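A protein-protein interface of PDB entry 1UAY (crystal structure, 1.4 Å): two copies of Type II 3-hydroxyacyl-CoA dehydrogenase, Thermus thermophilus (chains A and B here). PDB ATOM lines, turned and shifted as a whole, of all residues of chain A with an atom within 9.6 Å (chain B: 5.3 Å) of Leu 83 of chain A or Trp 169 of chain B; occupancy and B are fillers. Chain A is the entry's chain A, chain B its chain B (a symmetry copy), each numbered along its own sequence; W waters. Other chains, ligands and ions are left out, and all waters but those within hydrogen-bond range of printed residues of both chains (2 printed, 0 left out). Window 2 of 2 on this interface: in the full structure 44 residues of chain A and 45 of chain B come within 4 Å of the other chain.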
ATOM      1  N   GLU A  80     -11.874 -22.489   6.914  1.00  0.00           N
ATOM      2  CA  GLU A  80     -13.134 -22.810   6.256  1.00  0.00           C
ATOM      3  C   GLU A  80     -14.281 -22.712   7.248  1.00  0.00           C
ATOM      4  O   GLU A  80     -14.243 -23.308   8.325  1.00  0.00           O
ATOM      5  CB  GLU A  80     -13.077 -24.228   5.667  1.00  0.00           C
ATOM      6  CG  GLU A  80     -14.287 -24.588   4.806  1.00  0.00           C
ATOM      7  CD  GLU A  80     -14.178 -25.958   4.149  1.00  0.00           C
ATOM      8  OE1 GLU A  80     -13.084 -26.565   4.185  1.00  0.00           O
ATOM      9  OE2 GLU A  80     -15.188 -26.431   3.584  1.00  0.00           O
ATOM     10  N   LYS A  81     -15.307 -21.956   6.882  1.00  0.00           N
ATOM     11  CA  LYS A  81     -16.452 -21.783   7.761  1.00  0.00           C
ATOM     12  C   LYS A  81     -17.367 -22.998   7.772  1.00  0.00           C
ATOM     13  O   LYS A  81     -17.420 -23.768   6.810  1.00  0.00           O
ATOM     14  CB  LYS A  81     -17.249 -20.544   7.346  1.00  0.00           C
ATOM     15  CG  LYS A  81     -16.514 -19.235   7.598  1.00  0.00           C
ATOM     16  CD  LYS A  81     -17.349 -18.037   7.178  1.00  0.00           C
ATOM     17  CE  LYS A  81     -16.609 -16.738   7.451  1.00  0.00           C
ATOM     18  NZ  LYS A  81     -17.411 -15.548   7.061  1.00  0.00           N
ATOM     19  N   ILE A  82     -18.076 -23.170   8.880  1.00  0.00           N
ATOM     20  CA  ILE A  82     -19.024 -24.265   9.026  1.00  0.00           C
ATOM     21  C   ILE A  82     -20.144 -24.058   8.008  1.00  0.00           C
ATOM     22  O   ILE A  82     -20.616 -25.011   7.385  1.00  0.00           O
ATOM     23  CB  ILE A  82     -19.613 -24.289  10.454  1.00  0.00           C
ATOM     24  CG1 ILE A  82     -18.516 -24.676  11.448  1.00  0.00           C
ATOM     25  CG2 ILE A  82     -20.779 -25.267  10.530  1.00  0.00           C
ATOM     26  CD1 ILE A  82     -18.947 -24.625  12.894  1.00  0.00           C
ATOM     27  N   LEU A  83     -20.563 -22.808   7.846  1.00  0.00           N
ATOM     28  CA  LEU A  83     -21.613 -22.473   6.890  1.00  0.00           C
ATOM     29  C   LEU A  83     -21.012 -21.611   5.785  1.00  0.00           C
ATOM     30  O   LEU A  83     -20.731 -20.429   5.987  1.00  0.00           O
ATOM     31  CB  LEU A  83     -22.757 -21.727   7.589  1.00  0.00           C
ATOM     32  CG  LEU A  83     -23.410 -22.448   8.772  1.00  0.00           C
ATOM     33  CD1 LEU A  83     -24.551 -21.599   9.309  1.00  0.00           C
ATOM     34  CD2 LEU A  83     -23.914 -23.819   8.345  1.00  0.00           C
ATOM     35  N   GLY A  84     -20.804 -22.222   4.622  1.00  0.00           N
ATOM     36  CA  GLY A  84     -20.226 -21.515   3.492  1.00  0.00           C
ATOM     37  C   GLY A  84     -21.271 -20.810   2.651  1.00  0.00           C
ATOM     38  O   GLY A  84     -22.436 -20.728   3.034  1.00  0.00           O
ATOM     39  N   LYS A  85     -20.856 -20.305   1.496  1.00  0.00           N
ATOM     40  CA  LYS A  85     -21.771 -19.594   0.613  1.00  0.00           C
ATOM     41  C   LYS A  85     -22.611 -20.522  -0.260  1.00  0.00           C
ATOM     42  O   LYS A  85     -23.716 -20.162  -0.662  1.00  0.00           O
ATOM     43  CB  LYS A  85     -20.989 -18.613  -0.268  1.00  0.00           C
ATOM     44  CG  LYS A  85     -20.307 -17.493   0.509  1.00  0.00           C
ATOM     45  CD  LYS A  85     -21.325 -16.643   1.264  1.00  0.00           C
ATOM     46  CE  LYS A  85     -20.649 -15.535   2.060  1.00  0.00           C
ATOM     47  NZ  LYS A  85     -21.638 -14.673   2.771  1.00  0.00           N
ATOM     48  N   GLU A  86     -22.091 -21.713  -0.542  1.00  0.00           N
ATOM     49  CA  GLU A  86     -22.796 -22.686  -1.373  1.00  0.00           C
ATOM     50  C   GLU A  86     -23.374 -23.829  -0.545  1.00  0.00           C
ATOM     51  O   GLU A  86     -24.351 -24.466  -0.941  1.00  0.00           O
ATOM     52  CB  GLU A  86     -21.844 -23.268  -2.423  1.00  0.00           C
ATOM     53  CG  GLU A  86     -21.190 -22.243  -3.336  1.00  0.00           C
ATOM     54  CD  GLU A  86     -22.173 -21.591  -4.285  1.00  0.00           C
ATOM     55  OE1 GLU A  86     -23.088 -20.889  -3.806  1.00  0.00           O
ATOM     56  OE2 GLU A  86     -22.031 -21.780  -5.512  1.00  0.00           O
ATOM     57  N   GLY A  87     -22.758 -24.092   0.601  1.00  0.00           N
ATOM     58  CA  GLY A  87     -23.222 -25.164   1.459  1.00  0.00           C
ATOM     59  C   GLY A  87     -22.360 -25.268   2.700  1.00  0.00           C
ATOM     60  O   GLY A  87     -21.527 -24.400   2.947  1.00  0.00           O
ATOM     61  N   PRO A  88     -22.534 -26.326   3.499  1.00  0.00           N
ATOM     62  CA  PRO A  88     -21.740 -26.495   4.716  1.00  0.00           C
ATOM     63  C   PRO A  88     -20.297 -26.906   4.454  1.00  0.00           C
ATOM     64  O   PRO A  88     -19.945 -27.355   3.362  1.00  0.00           O
ATOM     65  CB  PRO A  88     -22.510 -27.569   5.477  1.00  0.00           C
ATOM     66  CG  PRO A  88     -23.049 -28.427   4.370  1.00  0.00           C
ATOM     67  CD  PRO A  88     -23.541 -27.396   3.373  1.00  0.00           C
ATOM     68  N   HIS A  89     -19.471 -26.729   5.479  1.00  0.00           N
ATOM     69  CA  HIS A  89     -18.058 -27.093   5.466  1.00  0.00           C
ATOM     70  C   HIS A  89     -17.954 -28.494   4.863  1.00  0.00           C
ATOM     71  O   HIS A  89     -18.717 -29.385   5.231  1.00  0.00           O
ATOM     72  CB  HIS A  89     -17.567 -27.103   6.919  1.00  0.00           C
ATOM     73  CG  HIS A  89     -16.083 -27.228   7.095  1.00  0.00           C
ATOM     74  ND1 HIS A  89     -15.352 -28.300   6.626  1.00  0.00           N
ATOM     75  CD2 HIS A  89     -15.212 -26.454   7.785  1.00  0.00           C
ATOM     76  CE1 HIS A  89     -14.097 -28.183   7.025  1.00  0.00           C
ATOM     77  NE2 HIS A  89     -13.986 -27.072   7.732  1.00  0.00           N
ATOM     78  N   GLY A  90     -17.023 -28.684   3.935  1.00  0.00           N
ATOM     79  CA  GLY A  90     -16.857 -29.989   3.327  1.00  0.00           C
ATOM     80  C   GLY A  90     -16.407 -31.024   4.342  1.00  0.00           C
ATOM     81  O   GLY A  90     -15.673 -30.715   5.280  1.00  0.00           O
ATOM     82  N   ILE A 143     -13.193 -18.134  14.240  1.00  0.00           N
ATOM     83  CA  ILE A 143     -14.184 -18.446  13.230  1.00  0.00           C
ATOM     84  C   ILE A 143     -13.411 -18.958  12.017  1.00  0.00           C
ATOM     85  O   ILE A 143     -12.419 -18.353  11.606  1.00  0.00           O
ATOM     86  CB  ILE A 143     -14.993 -17.186  12.860  1.00  0.00           C
ATOM     87  CG1 ILE A 143     -15.899 -16.803  14.033  1.00  0.00           C
ATOM     88  CG2 ILE A 143     -15.800 -17.427  11.591  1.00  0.00           C
ATOM     89  CD1 ILE A 143     -16.673 -15.509  13.826  1.00  0.00           C
ATOM     90  N   GLY A 144     -13.858 -20.086  11.473  1.00  0.00           N
ATOM     91  CA  GLY A 144     -13.202 -20.675  10.319  1.00  0.00           C
ATOM     92  C   GLY A 144     -12.140 -21.707  10.662  1.00  0.00           C
ATOM     93  O   GLY A 144     -11.586 -22.350   9.769  1.00  0.00           O
ATOM     94  N   ALA A 146     -12.614 -24.460  12.781  1.00  0.00           N
ATOM     95  CA  ALA A 146     -13.201 -25.634  13.413  1.00  0.00           C
ATOM     96  C   ALA A 146     -12.400 -26.918  13.192  1.00  0.00           C
ATOM     97  O   ALA A 146     -12.119 -27.649  14.145  1.00  0.00           O
ATOM     98  CB  ALA A 146     -14.633 -25.820  12.933  1.00  0.00           C
ATOM     99  N   ARG A 242     -12.412 -13.125  15.536  1.00  0.00           N
ATOM    100  CA  ARG A 242     -11.889 -12.737  14.230  1.00  0.00           C
ATOM    101  C   ARG A 242     -10.545 -12.040  14.394  1.00  0.00           C
ATOM    102  O   ARG A 242     -10.183 -11.731  15.550  1.00  0.00           O
ATOM    103  CB  ARG A 242     -12.866 -11.795  13.518  1.00  0.00           C
ATOM    104  CG  ARG A 242     -14.243 -12.385  13.264  1.00  0.00           C
ATOM    105  CD  ARG A 242     -15.124 -11.405  12.502  1.00  0.00           C
ATOM    106  NE  ARG A 242     -16.446 -11.954  12.215  1.00  0.00           N
ATOM    107  CZ  ARG A 242     -17.378 -12.190  13.133  1.00  0.00           C
ATOM    108  NH1 ARG A 242     -17.140 -11.921  14.411  1.00  0.00           N
ATOM    109  NH2 ARG A 242     -18.549 -12.696  12.775  1.00  0.00           N
ATOM    110  OXT ARG A 242      -9.876 -11.807  13.366  1.00  0.00           O
ATOM    111  N   ARG B 110     -22.413 -29.737  11.136  1.00  0.00           N
ATOM    112  CA  ARG B 110     -22.427 -28.942   9.913  1.00  0.00           C
ATOM    113  C   ARG B 110     -23.736 -29.066   9.135  1.00  0.00           C
ATOM    114  O   ARG B 110     -24.252 -28.074   8.612  1.00  0.00           O
ATOM    115  CB  ARG B 110     -21.242 -29.328   9.016  1.00  0.00           C
ATOM    116  CG  ARG B 110     -21.443 -30.615   8.249  1.00  0.00           C
ATOM    117  CD  ARG B 110     -20.178 -31.132   7.570  1.00  0.00           C
ATOM    118  NE  ARG B 110     -20.517 -32.350   6.840  1.00  0.00           N
ATOM    119  CZ  ARG B 110     -20.796 -32.403   5.541  1.00  0.00           C
ATOM    120  NH1 ARG B 110     -20.753 -31.307   4.796  1.00  0.00           N
ATOM    121  NH2 ARG B 110     -21.194 -33.547   5.003  1.00  0.00           N
ATOM    122  N   ALA B 113     -26.693 -27.476  11.330  1.00  0.00           N
ATOM    123  CA  ALA B 113     -26.562 -26.020  11.335  1.00  0.00           C
ATOM    124  C   ALA B 113     -27.024 -25.435  10.003  1.00  0.00           C
ATOM    125  O   ALA B 113     -27.729 -24.422   9.970  1.00  0.00           O
ATOM    126  CB  ALA B 113     -25.114 -25.619  11.612  1.00  0.00           C
ATOM    127  N   TRP B 114     -26.634 -26.069   8.903  1.00  0.00           N
ATOM    128  CA  TRP B 114     -27.038 -25.578   7.591  1.00  0.00           C
ATOM    129  C   TRP B 114     -28.559 -25.621   7.461  1.00  0.00           C
ATOM    130  O   TRP B 114     -29.178 -24.689   6.949  1.00  0.00           O
ATOM    131  CB  TRP B 114     -26.390 -26.413   6.483  1.00  0.00           C
ATOM    132  CG  TRP B 114     -26.675 -25.895   5.099  1.00  0.00           C
ATOM    133  CD1 TRP B 114     -27.630 -26.347   4.231  1.00  0.00           C
ATOM    134  CD2 TRP B 114     -26.023 -24.800   4.444  1.00  0.00           C
ATOM    135  NE1 TRP B 114     -27.611 -25.599   3.075  1.00  0.00           N
ATOM    136  CE2 TRP B 114     -26.636 -24.643   3.180  1.00  0.00           C
ATOM    137  CE3 TRP B 114     -24.979 -23.933   4.801  1.00  0.00           C
ATOM    138  CZ2 TRP B 114     -26.241 -23.650   2.270  1.00  0.00           C
ATOM    139  CZ3 TRP B 114     -24.586 -22.945   3.896  1.00  0.00           C
ATOM    140  CH2 TRP B 114     -25.218 -22.815   2.646  1.00  0.00           C
ATOM    141  N   ARG B 117     -30.157 -22.754   9.575  1.00  0.00           N
ATOM    142  CA  ARG B 117     -29.704 -21.394   9.309  1.00  0.00           C
ATOM    143  C   ARG B 117     -30.755 -20.393   8.846  1.00  0.00           C
ATOM    144  O   ARG B 117     -30.556 -19.185   8.985  1.00  0.00           O
ATOM    145  CB  ARG B 117     -28.538 -21.415   8.312  1.00  0.00           C
ATOM    146  CG  ARG B 117     -28.950 -21.519   6.860  1.00  0.00           C
ATOM    147  CD  ARG B 117     -27.733 -21.685   5.963  1.00  0.00           C
ATOM    148  NE  ARG B 117     -28.079 -21.520   4.555  1.00  0.00           N
ATOM    149  CZ  ARG B 117     -28.884 -22.331   3.876  1.00  0.00           C
ATOM    150  NH1 ARG B 117     -29.432 -23.384   4.469  1.00  0.00           N
ATOM    151  NH2 ARG B 117     -29.150 -22.080   2.601  1.00  0.00           N
ATOM    152  N   GLY B 125     -34.039 -15.151  20.009  1.00  0.00           N
ATOM    153  CA  GLY B 125     -33.168 -14.909  18.870  1.00  0.00           C
ATOM    154  C   GLY B 125     -32.467 -16.168  18.389  1.00  0.00           C
ATOM    155  O   GLY B 125     -31.543 -16.109  17.582  1.00  0.00           O
ATOM    156  N   ARG B 127     -32.098 -19.810  16.459  1.00  0.00           N
ATOM    157  CA  ARG B 127     -32.557 -20.570  15.305  1.00  0.00           C
ATOM    158  C   ARG B 127     -32.367 -22.050  15.635  1.00  0.00           C
ATOM    159  O   ARG B 127     -32.967 -22.920  15.005  1.00  0.00           O
ATOM    160  CB  ARG B 127     -31.772 -20.197  14.043  1.00  0.00           C
ATOM    161  CG  ARG B 127     -32.147 -18.834  13.467  1.00  0.00           C
ATOM    162  CD  ARG B 127     -31.650 -18.665  12.035  1.00  0.00           C
ATOM    163  NE  ARG B 127     -32.178 -17.451  11.410  1.00  0.00           N
ATOM    164  CZ  ARG B 127     -31.693 -16.229  11.602  1.00  0.00           C
ATOM    165  NH1 ARG B 127     -30.650 -16.040  12.402  1.00  0.00           N
ATOM    166  NH2 ARG B 127     -32.259 -15.188  11.006  1.00  0.00           N
ATOM    167  N   GLU B 165     -18.810 -18.801  15.270  1.00  0.00           N
ATOM    168  CA  GLU B 165     -19.328 -18.563  13.928  1.00  0.00           C
ATOM    169  C   GLU B 165     -20.844 -18.628  13.879  1.00  0.00           C
ATOM    170  O   GLU B 165     -21.501 -17.757  13.298  1.00  0.00           O
ATOM    171  CB  GLU B 165     -18.787 -19.596  12.945  1.00  0.00           C
ATOM    172  CG  GLU B 165     -19.247 -19.343  11.511  1.00  0.00           C
ATOM    173  CD  GLU B 165     -18.987 -20.515  10.594  1.00  0.00           C
ATOM    174  OE1 GLU B 165     -17.994 -21.235  10.823  1.00  0.00           O
ATOM    175  OE2 GLU B 165     -19.767 -20.705   9.631  1.00  0.00           O
ATOM    176  N   LEU B 166     -21.401 -19.664  14.491  1.00  0.00           N
ATOM    177  CA  LEU B 166     -22.838 -19.856  14.462  1.00  0.00           C
ATOM    178  C   LEU B 166     -23.612 -18.816  15.263  1.00  0.00           C
ATOM    179  O   LEU B 166     -24.827 -18.689  15.106  1.00  0.00           O
ATOM    180  CB  LEU B 166     -23.177 -21.278  14.913  1.00  0.00           C
ATOM    181  CG  LEU B 166     -22.617 -22.356  13.969  1.00  0.00           C
ATOM    182  CD1 LEU B 166     -23.041 -23.735  14.449  1.00  0.00           C
ATOM    183  CD2 LEU B 166     -23.105 -22.111  12.543  1.00  0.00           C
ATOM    184  N   ALA B 167     -22.904 -18.063  16.100  1.00  0.00           N
ATOM    185  CA  ALA B 167     -23.531 -17.016  16.901  1.00  0.00           C
ATOM    186  C   ALA B 167     -24.234 -16.025  15.976  1.00  0.00           C
ATOM    187  O   ALA B 167     -25.316 -15.528  16.291  1.00  0.00           O
ATOM    188  CB  ALA B 167     -22.482 -16.288  17.729  1.00  0.00           C
ATOM    189  N   GLY B 168     -23.608 -15.753  14.834  1.00  0.00           N
ATOM    190  CA  GLY B 168     -24.172 -14.821  13.875  1.00  0.00           C
ATOM    191  C   GLY B 168     -25.473 -15.308  13.271  1.00  0.00           C
ATOM    192  O   GLY B 168     -26.236 -14.519  12.711  1.00  0.00           O
ATOM    193  N   TRP B 169     -25.727 -16.609  13.381  1.00  0.00           N
ATOM    194  CA  TRP B 169     -26.947 -17.204  12.850  1.00  0.00           C
ATOM    195  C   TRP B 169     -27.934 -17.536  13.966  1.00  0.00           C
ATOM    196  O   TRP B 169     -29.010 -18.076  13.713  1.00  0.00           O
ATOM    197  CB  TRP B 169     -26.627 -18.491  12.080  1.00  0.00           C
ATOM    198  CG  TRP B 169     -25.682 -18.331  10.919  1.00  0.00           C
ATOM    199  CD1 TRP B 169     -24.315 -18.345  10.956  1.00  0.00           C
ATOM    200  CD2 TRP B 169     -26.044 -18.172   9.541  1.00  0.00           C
ATOM    201  NE1 TRP B 169     -23.803 -18.212   9.684  1.00  0.00           N
ATOM    202  CE2 TRP B 169     -24.843 -18.104   8.799  1.00  0.00           C
ATOM    203  CE3 TRP B 169     -27.266 -18.084   8.862  1.00  0.00           C
ATOM    204  CZ2 TRP B 169     -24.831 -17.952   7.406  1.00  0.00           C
ATOM    205  CZ3 TRP B 169     -27.253 -17.932   7.478  1.00  0.00           C
ATOM    206  CH2 TRP B 169     -26.042 -17.868   6.766  1.00  0.00           C
ATOM    207  N   GLY B 170     -27.565 -17.224  15.205  1.00  0.00           N
ATOM    208  CA  GLY B 170     -28.442 -17.523  16.324  1.00  0.00           C
ATOM    209  C   GLY B 170     -28.481 -19.003  16.670  1.00  0.00           C
ATOM    210  O   GLY B 170     -29.485 -19.509  17.161  1.00  0.00           O
ATOM    211  N   ILE B 171     -27.384 -19.708  16.406  1.00  0.00           N
ATOM    212  CA  ILE B 171     -27.312 -21.130  16.707  1.00  0.00           C
ATOM    213  C   ILE B 171     -26.227 -21.354  17.757  1.00  0.00           C
ATOM    214  O   ILE B 171     -25.073 -20.988  17.553  1.00  0.00           O
ATOM    215  CB  ILE B 171     -26.993 -21.946  15.433  1.00  0.00           C
ATOM    216  CG1 ILE B 171     -28.130 -21.774  14.417  1.00  0.00           C
ATOM    217  CG2 ILE B 171     -26.794 -23.421  15.785  1.00  0.00           C
ATOM    218  CD1 ILE B 171     -27.838 -22.385  13.056  1.00  0.00           C
HETATM  219  O   HOH W   1     -20.991 -18.671   8.561  1.00  0.00           O
HETATM  220  O   HOH W   2     -16.027 -21.584  12.632  1.00  0.00           O
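The guanidinium group of Arg 110 of chain B is in hydrogen-bond range of the backbone carbonyl oxygen of His 89 of chain A (2.8 Å).
N of Ile 82 of chain A lies within hydrogen-bond range of OE1 of Glu 165 of chain B.
The backbone NH (N) of Leu 83 of chain A sits at hydrogen-bond distance from the side-chain carboxylate (OE2) of Glu 165 of chain B, at 2.9 Å.
O of Leu 166 of chain B is in hydrogen-bond range of N of Ile 171 of chain B (3.0 Å).
The backbone carbonyl oxygen (O) of Trp 114 of chain B lies within hydrogen-bond range of the guanidinium group (NH1) of Arg 117 of chain B (2.8 Å).
NH1 of Arg 127 of chain B sits at hydrogen-bond distance from O of Trp 169 of chain B (2.9 Å).
The backbone NH (N) of His 89 of chain A sits at hydrogen-bond distance from the backbone carbonyl oxygen (O) of Ile 82 of chain A, at 2.8 Å.
Glu 165 of chain B touches Lys 81 of chain A.
Leu 83 of chain A touches Ala 113 of chain B.
Leu 83 of chain A touches Trp 114 of chain B (CD2 to N, 3.6 Å).
Leu 83 of chain A touches Leu 166 of chain B (CD1 to CD2, 3.6 Å).
O of Gly 84 of chain A touches CZ3 of Trp 114 of chain B, at 3.2 Å.
Glu 86 of chain A touches Trp 114 of chain B.
Gly 87 of chain A touches Trp 114 of chain B.
O of Arg 110 of chain B touches CB of Pro 88 of chain A (3.6 Å).
Pro 88 of chain A touches Trp 114 of chain B.
Ile 143 of chain A touches Glu 165 of chain B (CG1 to N, 3.7 Å).
Leu 83 of chain A touches just these residues of chain B: Ala 113, Trp 114, Glu 165, Leu 166 and Trp 169.
Lys 85 of chain A touches none of the printed residues of chain B.
Printed residues of chain B within 4 Å of Pro 88 of chain A: Arg 110 (3.6 Å) and Trp 114 (3.7 Å).
Ala 113 of chain B touches one residue of chain A.
Of the printed residues of chain A, Leu 166 of chain B touches Leu 83 (3.6 Å).
No residue of chain A comes within 4 Å of Ala 167 of chain B.
No residue of chain A comes within 4 Å of Gly 168 of chain B.
Of chain A, only Leu 83 (3.5 Å) comes within 4 Å of Trp 169 of chain B.
The nearest residue of chain B that does not touch Leu 83 of chain A is Arg 117 of chain B (4.1 Å).
The nearest printed residue of chain B that does not touch His 89 of chain A is Trp 114 of chain B (6.2 Å).
Hydrophobic or aromatic side chains of chain B that line the printed part of chain A: Ala 113, Trp 114, Leu 166 and Trp 169.
Of the 15 printed residues of chain A, 9 touch a printed residue of chain B.
Hydrophobic or aromatic side chains of chain A that line the printed part of chain B: Ile 82, Leu 83, Pro 88 and Ile 143.
Along chain A the printed residues that touch a printed residue of chain B span positions 81 to 143.
Among the printed residues, 14 pairs touch across the chains.
Among the printed residues, no Asp or Glu carboxylate lies within 4 Å of a Lys or Arg side-chain nitrogen of the other chain.
No position is printed for both chains.
Of the 14 pairs that touch across the chains among the printed residues, none has its exchanged pair printed and touching as well.
Water W1 lies within hydrogen-bond range of the side-chain carboxylate (OE2) of Glu 165 of chain B (2.6 Å), the indole nitrogen (NE1) of Trp 169 of chain B (3.1 Å) and the backbone carbonyl oxygen (O) of Leu 83 of chain A (3.1 Å).
Water W2 lies within hydrogen-bond range of the side-chain carboxylate of Glu 165 of chain B (2.7 Å) and the backbone NH of Gly 144 of chain A (2.9 Å).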
